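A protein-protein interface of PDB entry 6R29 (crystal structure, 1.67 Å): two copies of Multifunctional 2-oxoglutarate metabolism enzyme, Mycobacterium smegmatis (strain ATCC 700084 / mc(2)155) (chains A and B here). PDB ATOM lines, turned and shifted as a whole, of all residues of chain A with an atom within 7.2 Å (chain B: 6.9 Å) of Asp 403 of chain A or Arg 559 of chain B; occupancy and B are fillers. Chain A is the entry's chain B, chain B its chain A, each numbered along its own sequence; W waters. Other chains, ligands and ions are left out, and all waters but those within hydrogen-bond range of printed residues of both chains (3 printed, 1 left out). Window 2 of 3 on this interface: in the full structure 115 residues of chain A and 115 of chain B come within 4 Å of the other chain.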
ATOM      1  N   SER A 395       7.782  27.765 -23.689  1.00  0.00           N
ATOM      2  CA  SER A 395       7.704  26.616 -22.787  1.00  0.00           C
ATOM      3  C   SER A 395       8.979  25.761 -22.837  1.00  0.00           C
ATOM      4  O   SER A 395       9.207  24.989 -21.910  1.00  0.00           O
ATOM      5  CB  SER A 395       6.472  25.756 -23.084  1.00  0.00           C
ATOM      6  OG  SER A 395       6.497  25.202 -24.386  1.00  0.00           O
ATOM      7  N   MET A 396       9.841  25.935 -23.874  1.00  0.00           N
ATOM      8  CA  MET A 396      11.106  25.192 -23.932  1.00  0.00           C
ATOM      9  C   MET A 396      11.992  25.534 -22.729  1.00  0.00           C
ATOM     10  O   MET A 396      12.662  24.648 -22.199  1.00  0.00           O
ATOM     11  CB  MET A 396      11.873  25.523 -25.229  1.00  0.00           C
ATOM     12  CG  MET A 396      11.216  24.965 -26.474  1.00  0.00           C
ATOM     13  SD  MET A 396      12.224  25.538 -27.875  1.00  0.00           S
ATOM     14  CE  MET A 396      11.526  24.617 -29.149  1.00  0.00           C
ATOM     15  N   GLN A 398      10.808  28.000 -20.087  1.00  0.00           N
ATOM     16  CA  GLN A 398       9.983  28.365 -18.929  1.00  0.00           C
ATOM     17  C   GLN A 398       8.735  27.478 -18.894  1.00  0.00           C
ATOM     18  O   GLN A 398       7.615  27.989 -19.007  1.00  0.00           O
ATOM     19  CB  GLN A 398       9.595  29.852 -18.988  1.00  0.00           C
ATOM     20  CG  GLN A 398      10.636  30.791 -18.388  1.00  0.00           C
ATOM     21  CD  GLN A 398      11.824  31.026 -19.279  1.00  0.00           C
ATOM     22  OE1 GLN A 398      11.712  31.143 -20.512  1.00  0.00           O
ATOM     23  NE2 GLN A 398      13.003  31.110 -18.660  1.00  0.00           N
ATOM     24  N   PRO A 399       8.897  26.137 -18.757  1.00  0.00           N
ATOM     25  CA  PRO A 399       7.710  25.260 -18.821  1.00  0.00           C
ATOM     26  C   PRO A 399       6.717  25.523 -17.694  1.00  0.00           C
ATOM     27  O   PRO A 399       5.509  25.524 -17.955  1.00  0.00           O
ATOM     28  CB  PRO A 399       8.305  23.838 -18.721  1.00  0.00           C
ATOM     29  CG  PRO A 399       9.661  24.031 -18.056  1.00  0.00           C
ATOM     30  CD  PRO A 399      10.146  25.351 -18.629  1.00  0.00           C
ATOM     31  N   TYR A 400       7.211  25.767 -16.468  1.00  0.00           N
ATOM     32  CA  TYR A 400       6.332  25.981 -15.304  1.00  0.00           C
ATOM     33  C   TYR A 400       5.544  27.285 -15.436  1.00  0.00           C
ATOM     34  O   TYR A 400       4.322  27.292 -15.270  1.00  0.00           O
ATOM     35  CB  TYR A 400       7.136  25.984 -13.994  1.00  0.00           C
ATOM     36  CG  TYR A 400       6.246  26.155 -12.780  1.00  0.00           C
ATOM     37  CD1 TYR A 400       5.259  25.221 -12.477  1.00  0.00           C
ATOM     38  CD2 TYR A 400       6.372  27.263 -11.951  1.00  0.00           C
ATOM     39  CE1 TYR A 400       4.403  25.397 -11.389  1.00  0.00           C
ATOM     40  CE2 TYR A 400       5.538  27.436 -10.841  1.00  0.00           C
ATOM     41  CZ  TYR A 400       4.556  26.497 -10.566  1.00  0.00           C
ATOM     42  OH  TYR A 400       3.725  26.645  -9.482  1.00  0.00           O
ATOM     43  N   MET A 401       6.237  28.374 -15.775  1.00  0.00           N
ATOM     44  CA  MET A 401       5.569  29.662 -15.946  1.00  0.00           C
ATOM     45  C   MET A 401       4.445  29.562 -16.990  1.00  0.00           C
ATOM     46  O   MET A 401       3.355  30.086 -16.762  1.00  0.00           O
ATOM     47  CB  MET A 401       6.601  30.740 -16.356  1.00  0.00           C
ATOM     48  CG  MET A 401       5.958  32.050 -16.787  1.00  0.00           C
ATOM     49  SD  MET A 401       7.152  33.299 -17.331  1.00  0.00           S
ATOM     50  CE  MET A 401       7.728  33.892 -15.756  1.00  0.00           C
ATOM     51  N   TYR A 402       4.677  28.851 -18.104  1.00  0.00           N
ATOM     52  CA  TYR A 402       3.680  28.815 -19.170  1.00  0.00           C
ATOM     53  C   TYR A 402       2.583  27.812 -18.852  1.00  0.00           C
ATOM     54  O   TYR A 402       1.455  28.018 -19.309  1.00  0.00           O
ATOM     55  CB  TYR A 402       4.330  28.635 -20.555  1.00  0.00           C
ATOM     56  CG  TYR A 402       4.787  30.021 -20.948  1.00  0.00           C
ATOM     57  CD1 TYR A 402       3.904  30.918 -21.551  1.00  0.00           C
ATOM     58  CD2 TYR A 402       6.007  30.523 -20.491  1.00  0.00           C
ATOM     59  CE1 TYR A 402       4.241  32.261 -21.732  1.00  0.00           C
ATOM     60  CE2 TYR A 402       6.345  31.867 -20.645  1.00  0.00           C
ATOM     61  CZ  TYR A 402       5.469  32.723 -21.296  1.00  0.00           C
ATOM     62  OH  TYR A 402       5.795  34.040 -21.452  1.00  0.00           O
ATOM     63  N   ASP A 403       2.839  26.848 -17.953  1.00  0.00           N
ATOM     64  CA  ASP A 403       1.754  25.977 -17.500  1.00  0.00           C
ATOM     65  C   ASP A 403       0.803  26.804 -16.615  1.00  0.00           C
ATOM     66  O   ASP A 403      -0.405  26.652 -16.734  1.00  0.00           O
ATOM     67  CB  ASP A 403       2.287  24.749 -16.748  1.00  0.00           C
ATOM     68  CG  ASP A 403       2.803  23.655 -17.664  1.00  0.00           C
ATOM     69  OD1 ASP A 403       2.425  23.648 -18.861  1.00  0.00           O
ATOM     70  OD2 ASP A 403       3.569  22.800 -17.184  1.00  0.00           O
ATOM     71  N   VAL A 404       1.353  27.723 -15.793  1.00  0.00           N
ATOM     72  CA  VAL A 404       0.552  28.610 -14.935  1.00  0.00           C
ATOM     73  C   VAL A 404      -0.190  29.640 -15.807  1.00  0.00           C
ATOM     74  O   VAL A 404      -1.402  29.831 -15.628  1.00  0.00           O
ATOM     75  CB  VAL A 404       1.404  29.287 -13.836  1.00  0.00           C
ATOM     76  CG1 VAL A 404       0.594  30.338 -13.059  1.00  0.00           C
ATOM     77  CG2 VAL A 404       1.988  28.239 -12.877  1.00  0.00           C
ATOM     78  N   ILE A 405       0.513  30.264 -16.785  1.00  0.00           N
ATOM     79  CA  ILE A 405      -0.132  31.249 -17.668  1.00  0.00           C
ATOM     80  C   ILE A 405      -1.316  30.633 -18.414  1.00  0.00           C
ATOM     81  O   ILE A 405      -2.347  31.300 -18.539  1.00  0.00           O
ATOM     82  CB  ILE A 405       0.901  31.884 -18.627  1.00  0.00           C
ATOM     83  CG1 ILE A 405       1.803  32.834 -17.821  1.00  0.00           C
ATOM     84  CG2 ILE A 405       0.225  32.602 -19.827  1.00  0.00           C
ATOM     85  CD1 ILE A 405       3.047  33.368 -18.557  1.00  0.00           C
ATOM     86  N   ASP A 406      -1.205  29.359 -18.848  1.00  0.00           N
ATOM     87  CA  ASP A 406      -2.275  28.656 -19.560  1.00  0.00           C
ATOM     88  C   ASP A 406      -3.568  28.498 -18.724  1.00  0.00           C
ATOM     89  O   ASP A 406      -4.635  28.335 -19.309  1.00  0.00           O
ATOM     90  CB  ASP A 406      -1.782  27.280 -20.040  1.00  0.00           C
ATOM     91  CG  ASP A 406      -0.781  27.341 -21.189  1.00  0.00           C
ATOM     92  OD1 ASP A 406      -0.577  28.453 -21.754  1.00  0.00           O
ATOM     93  OD2 ASP A 406      -0.174  26.290 -21.507  1.00  0.00           O
ATOM     94  N   THR A 407      -3.483  28.581 -17.389  1.00  0.00           N
ATOM     95  CA  THR A 407      -4.647  28.461 -16.485  1.00  0.00           C
ATOM     96  C   THR A 407      -5.294  29.817 -16.187  1.00  0.00           C
ATOM     97  O   THR A 407      -6.367  29.857 -15.585  1.00  0.00           O
ATOM     98  CB  THR A 407      -4.248  27.818 -15.135  1.00  0.00           C
ATOM     99  OG1 THR A 407      -3.512  28.757 -14.333  1.00  0.00           O
ATOM    100  CG2 THR A 407      -3.499  26.504 -15.286  1.00  0.00           C
ATOM    101  N   LYS A 408      -4.625  30.918 -16.557  1.00  0.00           N
ATOM    102  CA  LYS A 408      -5.062  32.269 -16.223  1.00  0.00           C
ATOM    103  C   LYS A 408      -6.062  32.861 -17.195  1.00  0.00           C
ATOM    104  O   LYS A 408      -5.814  32.912 -18.404  1.00  0.00           O
ATOM    105  CB  LYS A 408      -3.853  33.236 -16.148  1.00  0.00           C
ATOM    106  CG  LYS A 408      -2.927  33.013 -14.964  1.00  0.00           C
ATOM    107  CD  LYS A 408      -2.794  34.261 -14.122  1.00  0.00           C
ATOM    108  CE  LYS A 408      -3.867  34.318 -13.065  1.00  0.00           C
ATOM    109  NZ  LYS A 408      -3.969  35.669 -12.473  1.00  0.00           N
ATOM    110  N   PHE B 495      14.272  12.028 -16.865  1.00  0.00           N
ATOM    111  CA  PHE B 495      14.246  13.375 -17.469  1.00  0.00           C
ATOM    112  C   PHE B 495      13.215  13.439 -18.593  1.00  0.00           C
ATOM    113  O   PHE B 495      13.190  12.547 -19.443  1.00  0.00           O
ATOM    114  CB  PHE B 495      15.640  13.756 -18.011  1.00  0.00           C
ATOM    115  CG  PHE B 495      15.841  15.239 -18.250  1.00  0.00           C
ATOM    116  CD1 PHE B 495      15.466  15.825 -19.456  1.00  0.00           C
ATOM    117  CD2 PHE B 495      16.417  16.044 -17.275  1.00  0.00           C
ATOM    118  CE1 PHE B 495      15.646  17.201 -19.673  1.00  0.00           C
ATOM    119  CE2 PHE B 495      16.615  17.413 -17.500  1.00  0.00           C
ATOM    120  CZ  PHE B 495      16.236  17.977 -18.702  1.00  0.00           C
ATOM    121  N   THR B 496      12.349  14.489 -18.588  1.00  0.00           N
ATOM    122  CA  THR B 496      11.338  14.674 -19.629  1.00  0.00           C
ATOM    123  C   THR B 496      11.798  15.800 -20.561  1.00  0.00           C
ATOM    124  O   THR B 496      11.838  16.958 -20.139  1.00  0.00           O
ATOM    125  CB  THR B 496       9.955  14.981 -19.007  1.00  0.00           C
ATOM    126  OG1 THR B 496       9.622  13.968 -18.057  1.00  0.00           O
ATOM    127  CG2 THR B 496       8.855  15.094 -20.057  1.00  0.00           C
ATOM    128  N   VAL B 497      12.141  15.464 -21.810  1.00  0.00           N
ATOM    129  CA  VAL B 497      12.574  16.480 -22.781  1.00  0.00           C
ATOM    130  C   VAL B 497      11.346  17.154 -23.373  1.00  0.00           C
ATOM    131  O   VAL B 497      10.346  16.476 -23.669  1.00  0.00           O
ATOM    132  CB  VAL B 497      13.473  15.897 -23.908  1.00  0.00           C
ATOM    133  CG1 VAL B 497      14.012  17.012 -24.823  1.00  0.00           C
ATOM    134  CG2 VAL B 497      14.625  15.088 -23.321  1.00  0.00           C
ATOM    135  N   HIS B 498      11.417  18.490 -23.551  1.00  0.00           N
ATOM    136  CA  HIS B 498      10.349  19.236 -24.212  1.00  0.00           C
ATOM    137  C   HIS B 498      10.137  18.611 -25.594  1.00  0.00           C
ATOM    138  O   HIS B 498      11.127  18.309 -26.274  1.00  0.00           O
ATOM    139  CB  HIS B 498      10.736  20.715 -24.330  1.00  0.00           C
ATOM    140  CG  HIS B 498       9.636  21.583 -24.855  1.00  0.00           C
ATOM    141  ND1 HIS B 498       9.331  21.626 -26.208  1.00  0.00           N
ATOM    142  CD2 HIS B 498       8.825  22.443 -24.195  1.00  0.00           C
ATOM    143  CE1 HIS B 498       8.356  22.512 -26.329  1.00  0.00           C
ATOM    144  NE2 HIS B 498       8.016  23.028 -25.145  1.00  0.00           N
ATOM    145  N   PRO B 499       8.881  18.351 -26.017  1.00  0.00           N
ATOM    146  CA  PRO B 499       8.670  17.650 -27.300  1.00  0.00           C
ATOM    147  C   PRO B 499       9.224  18.370 -28.529  1.00  0.00           C
ATOM    148  O   PRO B 499       9.495  17.696 -29.519  1.00  0.00           O
ATOM    149  CB  PRO B 499       7.140  17.487 -27.390  1.00  0.00           C
ATOM    150  CG  PRO B 499       6.579  18.436 -26.413  1.00  0.00           C
ATOM    151  CD  PRO B 499       7.601  18.610 -25.324  1.00  0.00           C
ATOM    152  N   ARG B 500       9.462  19.692 -28.466  1.00  0.00           N
ATOM    153  CA  ARG B 500      10.024  20.393 -29.621  1.00  0.00           C
ATOM    154  C   ARG B 500      11.565  20.542 -29.507  1.00  0.00           C
ATOM    155  O   ARG B 500      12.220  21.016 -30.443  1.00  0.00           O
ATOM    156  CB  ARG B 500       9.298  21.722 -29.860  1.00  0.00           C
ATOM    157  CG  ARG B 500       7.840  21.404 -30.253  1.00  0.00           C
ATOM    158  CD  ARG B 500       6.940  22.564 -30.633  1.00  0.00           C
ATOM    159  NE  ARG B 500       6.535  23.395 -29.497  1.00  0.00           N
ATOM    160  CZ  ARG B 500       5.646  23.065 -28.561  1.00  0.00           C
ATOM    161  NH1 ARG B 500       5.356  23.917 -27.586  1.00  0.00           N
ATOM    162  NH2 ARG B 500       5.060  21.872 -28.578  1.00  0.00           N
ATOM    163  N   VAL B 557      15.788  22.002 -20.517  1.00  0.00           N
ATOM    164  CA  VAL B 557      14.996  22.127 -19.294  1.00  0.00           C
ATOM    165  C   VAL B 557      13.932  21.036 -19.247  1.00  0.00           C
ATOM    166  O   VAL B 557      13.185  20.859 -20.207  1.00  0.00           O
ATOM    167  CB  VAL B 557      14.369  23.557 -19.220  1.00  0.00           C
ATOM    168  CG1 VAL B 557      13.503  23.720 -17.969  1.00  0.00           C
ATOM    169  CG2 VAL B 557      15.447  24.651 -19.280  1.00  0.00           C
ATOM    170  N   ASP B 558      13.869  20.301 -18.124  1.00  0.00           N
ATOM    171  CA  ASP B 558      12.896  19.238 -17.912  1.00  0.00           C
ATOM    172  C   ASP B 558      11.487  19.837 -17.980  1.00  0.00           C
ATOM    173  O   ASP B 558      11.190  20.778 -17.249  1.00  0.00           O
ATOM    174  CB  ASP B 558      13.144  18.538 -16.564  1.00  0.00           C
ATOM    175  CG  ASP B 558      12.278  17.304 -16.361  1.00  0.00           C
ATOM    176  OD1 ASP B 558      11.033  17.445 -16.332  1.00  0.00           O
ATOM    177  OD2 ASP B 558      12.840  16.205 -16.221  1.00  0.00           O
ATOM    178  N   ARG B 559      10.653  19.329 -18.897  1.00  0.00           N
ATOM    179  CA  ARG B 559       9.303  19.852 -19.168  1.00  0.00           C
ATOM    180  C   ARG B 559       8.388  19.747 -17.944  1.00  0.00           C
ATOM    181  O   ARG B 559       7.453  20.550 -17.814  1.00  0.00           O
ATOM    182  CB  ARG B 559       8.682  19.111 -20.381  1.00  0.00           C
ATOM    183  CG  ARG B 559       7.280  19.559 -20.829  1.00  0.00           C
ATOM    184  CD  ARG B 559       7.189  21.008 -21.285  1.00  0.00           C
ATOM    185  NE  ARG B 559       5.802  21.419 -21.549  1.00  0.00           N
ATOM    186  CZ  ARG B 559       4.927  21.777 -20.610  1.00  0.00           C
ATOM    187  NH1 ARG B 559       5.274  21.767 -19.326  1.00  0.00           N
ATOM    188  NH2 ARG B 559       3.692  22.129 -20.946  1.00  0.00           N
ATOM    189  N   LYS B 560       8.657  18.776 -17.053  1.00  0.00           N
ATOM    190  CA  LYS B 560       7.807  18.542 -15.885  1.00  0.00           C
ATOM    191  C   LYS B 560       8.344  19.149 -14.597  1.00  0.00           C
ATOM    192  O   LYS B 560       7.538  19.500 -13.729  1.00  0.00           O
ATOM    193  CB  LYS B 560       7.607  17.029 -15.663  1.00  0.00           C
ATOM    194  CG  LYS B 560       6.725  16.362 -16.708  1.00  0.00           C
ATOM    195  CD  LYS B 560       6.496  14.895 -16.350  1.00  0.00           C
ATOM    196  CE  LYS B 560       5.774  14.140 -17.435  1.00  0.00           C
ATOM    197  NZ  LYS B 560       5.611  12.703 -17.083  1.00  0.00           N
ATOM    198  N   THR B 561       9.679  19.223 -14.428  1.00  0.00           N
ATOM    199  CA  THR B 561      10.277  19.673 -13.165  1.00  0.00           C
ATOM    200  C   THR B 561      11.099  20.949 -13.246  1.00  0.00           C
ATOM    201  O   THR B 561      11.468  21.494 -12.199  1.00  0.00           O
ATOM    202  CB  THR B 561      11.196  18.571 -12.584  1.00  0.00           C
ATOM    203  OG1 THR B 561      12.364  18.452 -13.398  1.00  0.00           O
ATOM    204  CG2 THR B 561      10.505  17.223 -12.440  1.00  0.00           C
ATOM    205  N   GLY B 562      11.471  21.369 -14.456  1.00  0.00           N
ATOM    206  CA  GLY B 562      12.313  22.549 -14.614  1.00  0.00           C
ATOM    207  C   GLY B 562      13.790  22.283 -14.376  1.00  0.00           C
ATOM    208  O   GLY B 562      14.595  23.207 -14.479  1.00  0.00           O
ATOM    209  N   GLU B 563      14.167  21.020 -14.061  1.00  0.00           N
ATOM    210  CA  GLU B 563      15.573  20.637 -13.850  1.00  0.00           C
ATOM    211  C   GLU B 563      16.361  20.819 -15.145  1.00  0.00           C
ATOM    212  O   GLU B 563      15.825  20.604 -16.232  1.00  0.00           O
ATOM    213  CB  GLU B 563      15.687  19.194 -13.364  1.00  0.00           C
ATOM    214  CG  GLU B 563      15.293  19.024 -11.906  1.00  0.00           C
ATOM    215  CD  GLU B 563      15.133  17.574 -11.496  1.00  0.00           C
ATOM    216  OE1 GLU B 563      14.118  16.954 -11.888  1.00  0.00           O
ATOM    217  OE2 GLU B 563      16.028  17.054 -10.790  1.00  0.00           O
HETATM  218  O   HOH W   1      14.578  22.746 -23.040  1.00  0.00           O
HETATM  219  O   HOH W   2       4.384  24.906 -20.496  1.00  0.00           O
HETATM  220  O   HOH W   3       7.142  22.431 -15.425  1.00  0.00           O
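The side-chain carboxylate (OD2) of Asp 558 of chain B is in hydrogen-bond range of the backbone NH (N) of Thr 496 of chain B, 3.0 Å away.
The backbone carbonyl oxygen (O) of Thr 496 of chain B lies within hydrogen-bond range of the backbone NH (N) of Arg 559 of chain B, 2.9 Å away.
A ring nitrogen (ND1) of His 498 of chain B is in hydrogen-bond range of the backbone NH of Arg 500 of chain B (3.0 Å).
OD1 of Asp 558 of chain B lies within hydrogen-bond range of N of Lys 560 of chain B.
OD1 of Asp 558 of chain B lies within hydrogen-bond range of N of Thr 561 of chain B (2.9 Å).
N of Asp 558 of chain B is in hydrogen-bond range of O of Glu 563 of chain B (2.7 Å).
Among the printed residues, merely in contact across the chains: Pro 399 of chain A with Arg 559 of chain B (3.5 Å), Met 396 of chain A with His 498 of chain B (3.6 Å), Met 396 of chain A with Val 557 of chain B (3.6 Å), Ser 395 of chain A with Arg 500 of chain B (3.6 Å), Pro 399 of chain A with Asp 558 of chain B (3.7 Å), Met 396 of chain A with Arg 500 of chain B (3.7 Å) and Pro 399 of chain A with Val 557 of chain B (3.8 Å).
A ring nitrogen (NE2) of His 498 of chain B lies within hydrogen-bond range of the side-chain hydroxyl (OG) of Ser 395 of chain A, 2.8 Å away.
The guanidinium group of Arg 559 of chain B lies within salt-bridge range of the side-chain carboxylate of Asp 403 of chain A.
Water W1 bridges the backbone carbonyl oxygen of Met 396 of chain A (2.8 Å) and the backbone NH of Val 557 of chain B (2.9 Å).
Water W2 lies within hydrogen-bond range of the side-chain carboxylate of Asp 403 of chain A (2.8 Å), the backbone carbonyl oxygen of Pro 399 of chain A (2.8 Å) and the guanidinium group of Arg 559 of chain B (2.9 Å).
Water W3 lies within hydrogen-bond range of the backbone carbonyl oxygen (O) of Arg 559 of chain B, the backbone carbonyl oxygen (O) of Lys 560 of chain B and the backbone NH (N) of Tyr 400 of chain A.
Of the 13 printed residues of chain B, 5 touch a printed residue of chain A.
Hydrophobic or aromatic side chains of chain B that line the printed part of chain A: His 498 and Val 557.
Of the 13 printed residues of chain A, 4 touch a printed residue of chain B.
Hydrophobic or aromatic side chains of chain A within 4 Å of the printed part of chain B: Met 396 and Pro 399.
Of the printed residues of chain B, Met 396 of chain A touches His 498, Arg 500 and Val 557.
Printed residues of chain B within 4 Å of Pro 399 of chain A: Val 557 (3.8 Å), Asp 558 (3.7 Å) and Arg 559 (3.5 Å).
Asp 403 of chain A touches one residue of chain B.
Printed residues of chain A within 4 Å of Val 557 of chain B: Met 396 and Pro 399.
Arg 559 of chain B touches just these residues of chain A: Pro 399 (3.5 Å) and Asp 403 (2.9 Å).
Gly 562 of chain B touches none of the printed residues of chain A.
The nearest residue of chain B that does not touch Asp 403 of chain A is Lys 560 of chain B (6.1 Å).
The nearest residue of chain A that does not touch Arg 559 of chain B is Ser 395 of chain A (4.5 Å).
The nearest printed residue of chain A that does not touch Val 557 of chain B is Gln 398 of chain A (5.5 Å).
No position is printed for both chains.
Of the 9 pairs that touch across the chains among the printed residues, none has its exchanged pair printed and touching as well.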
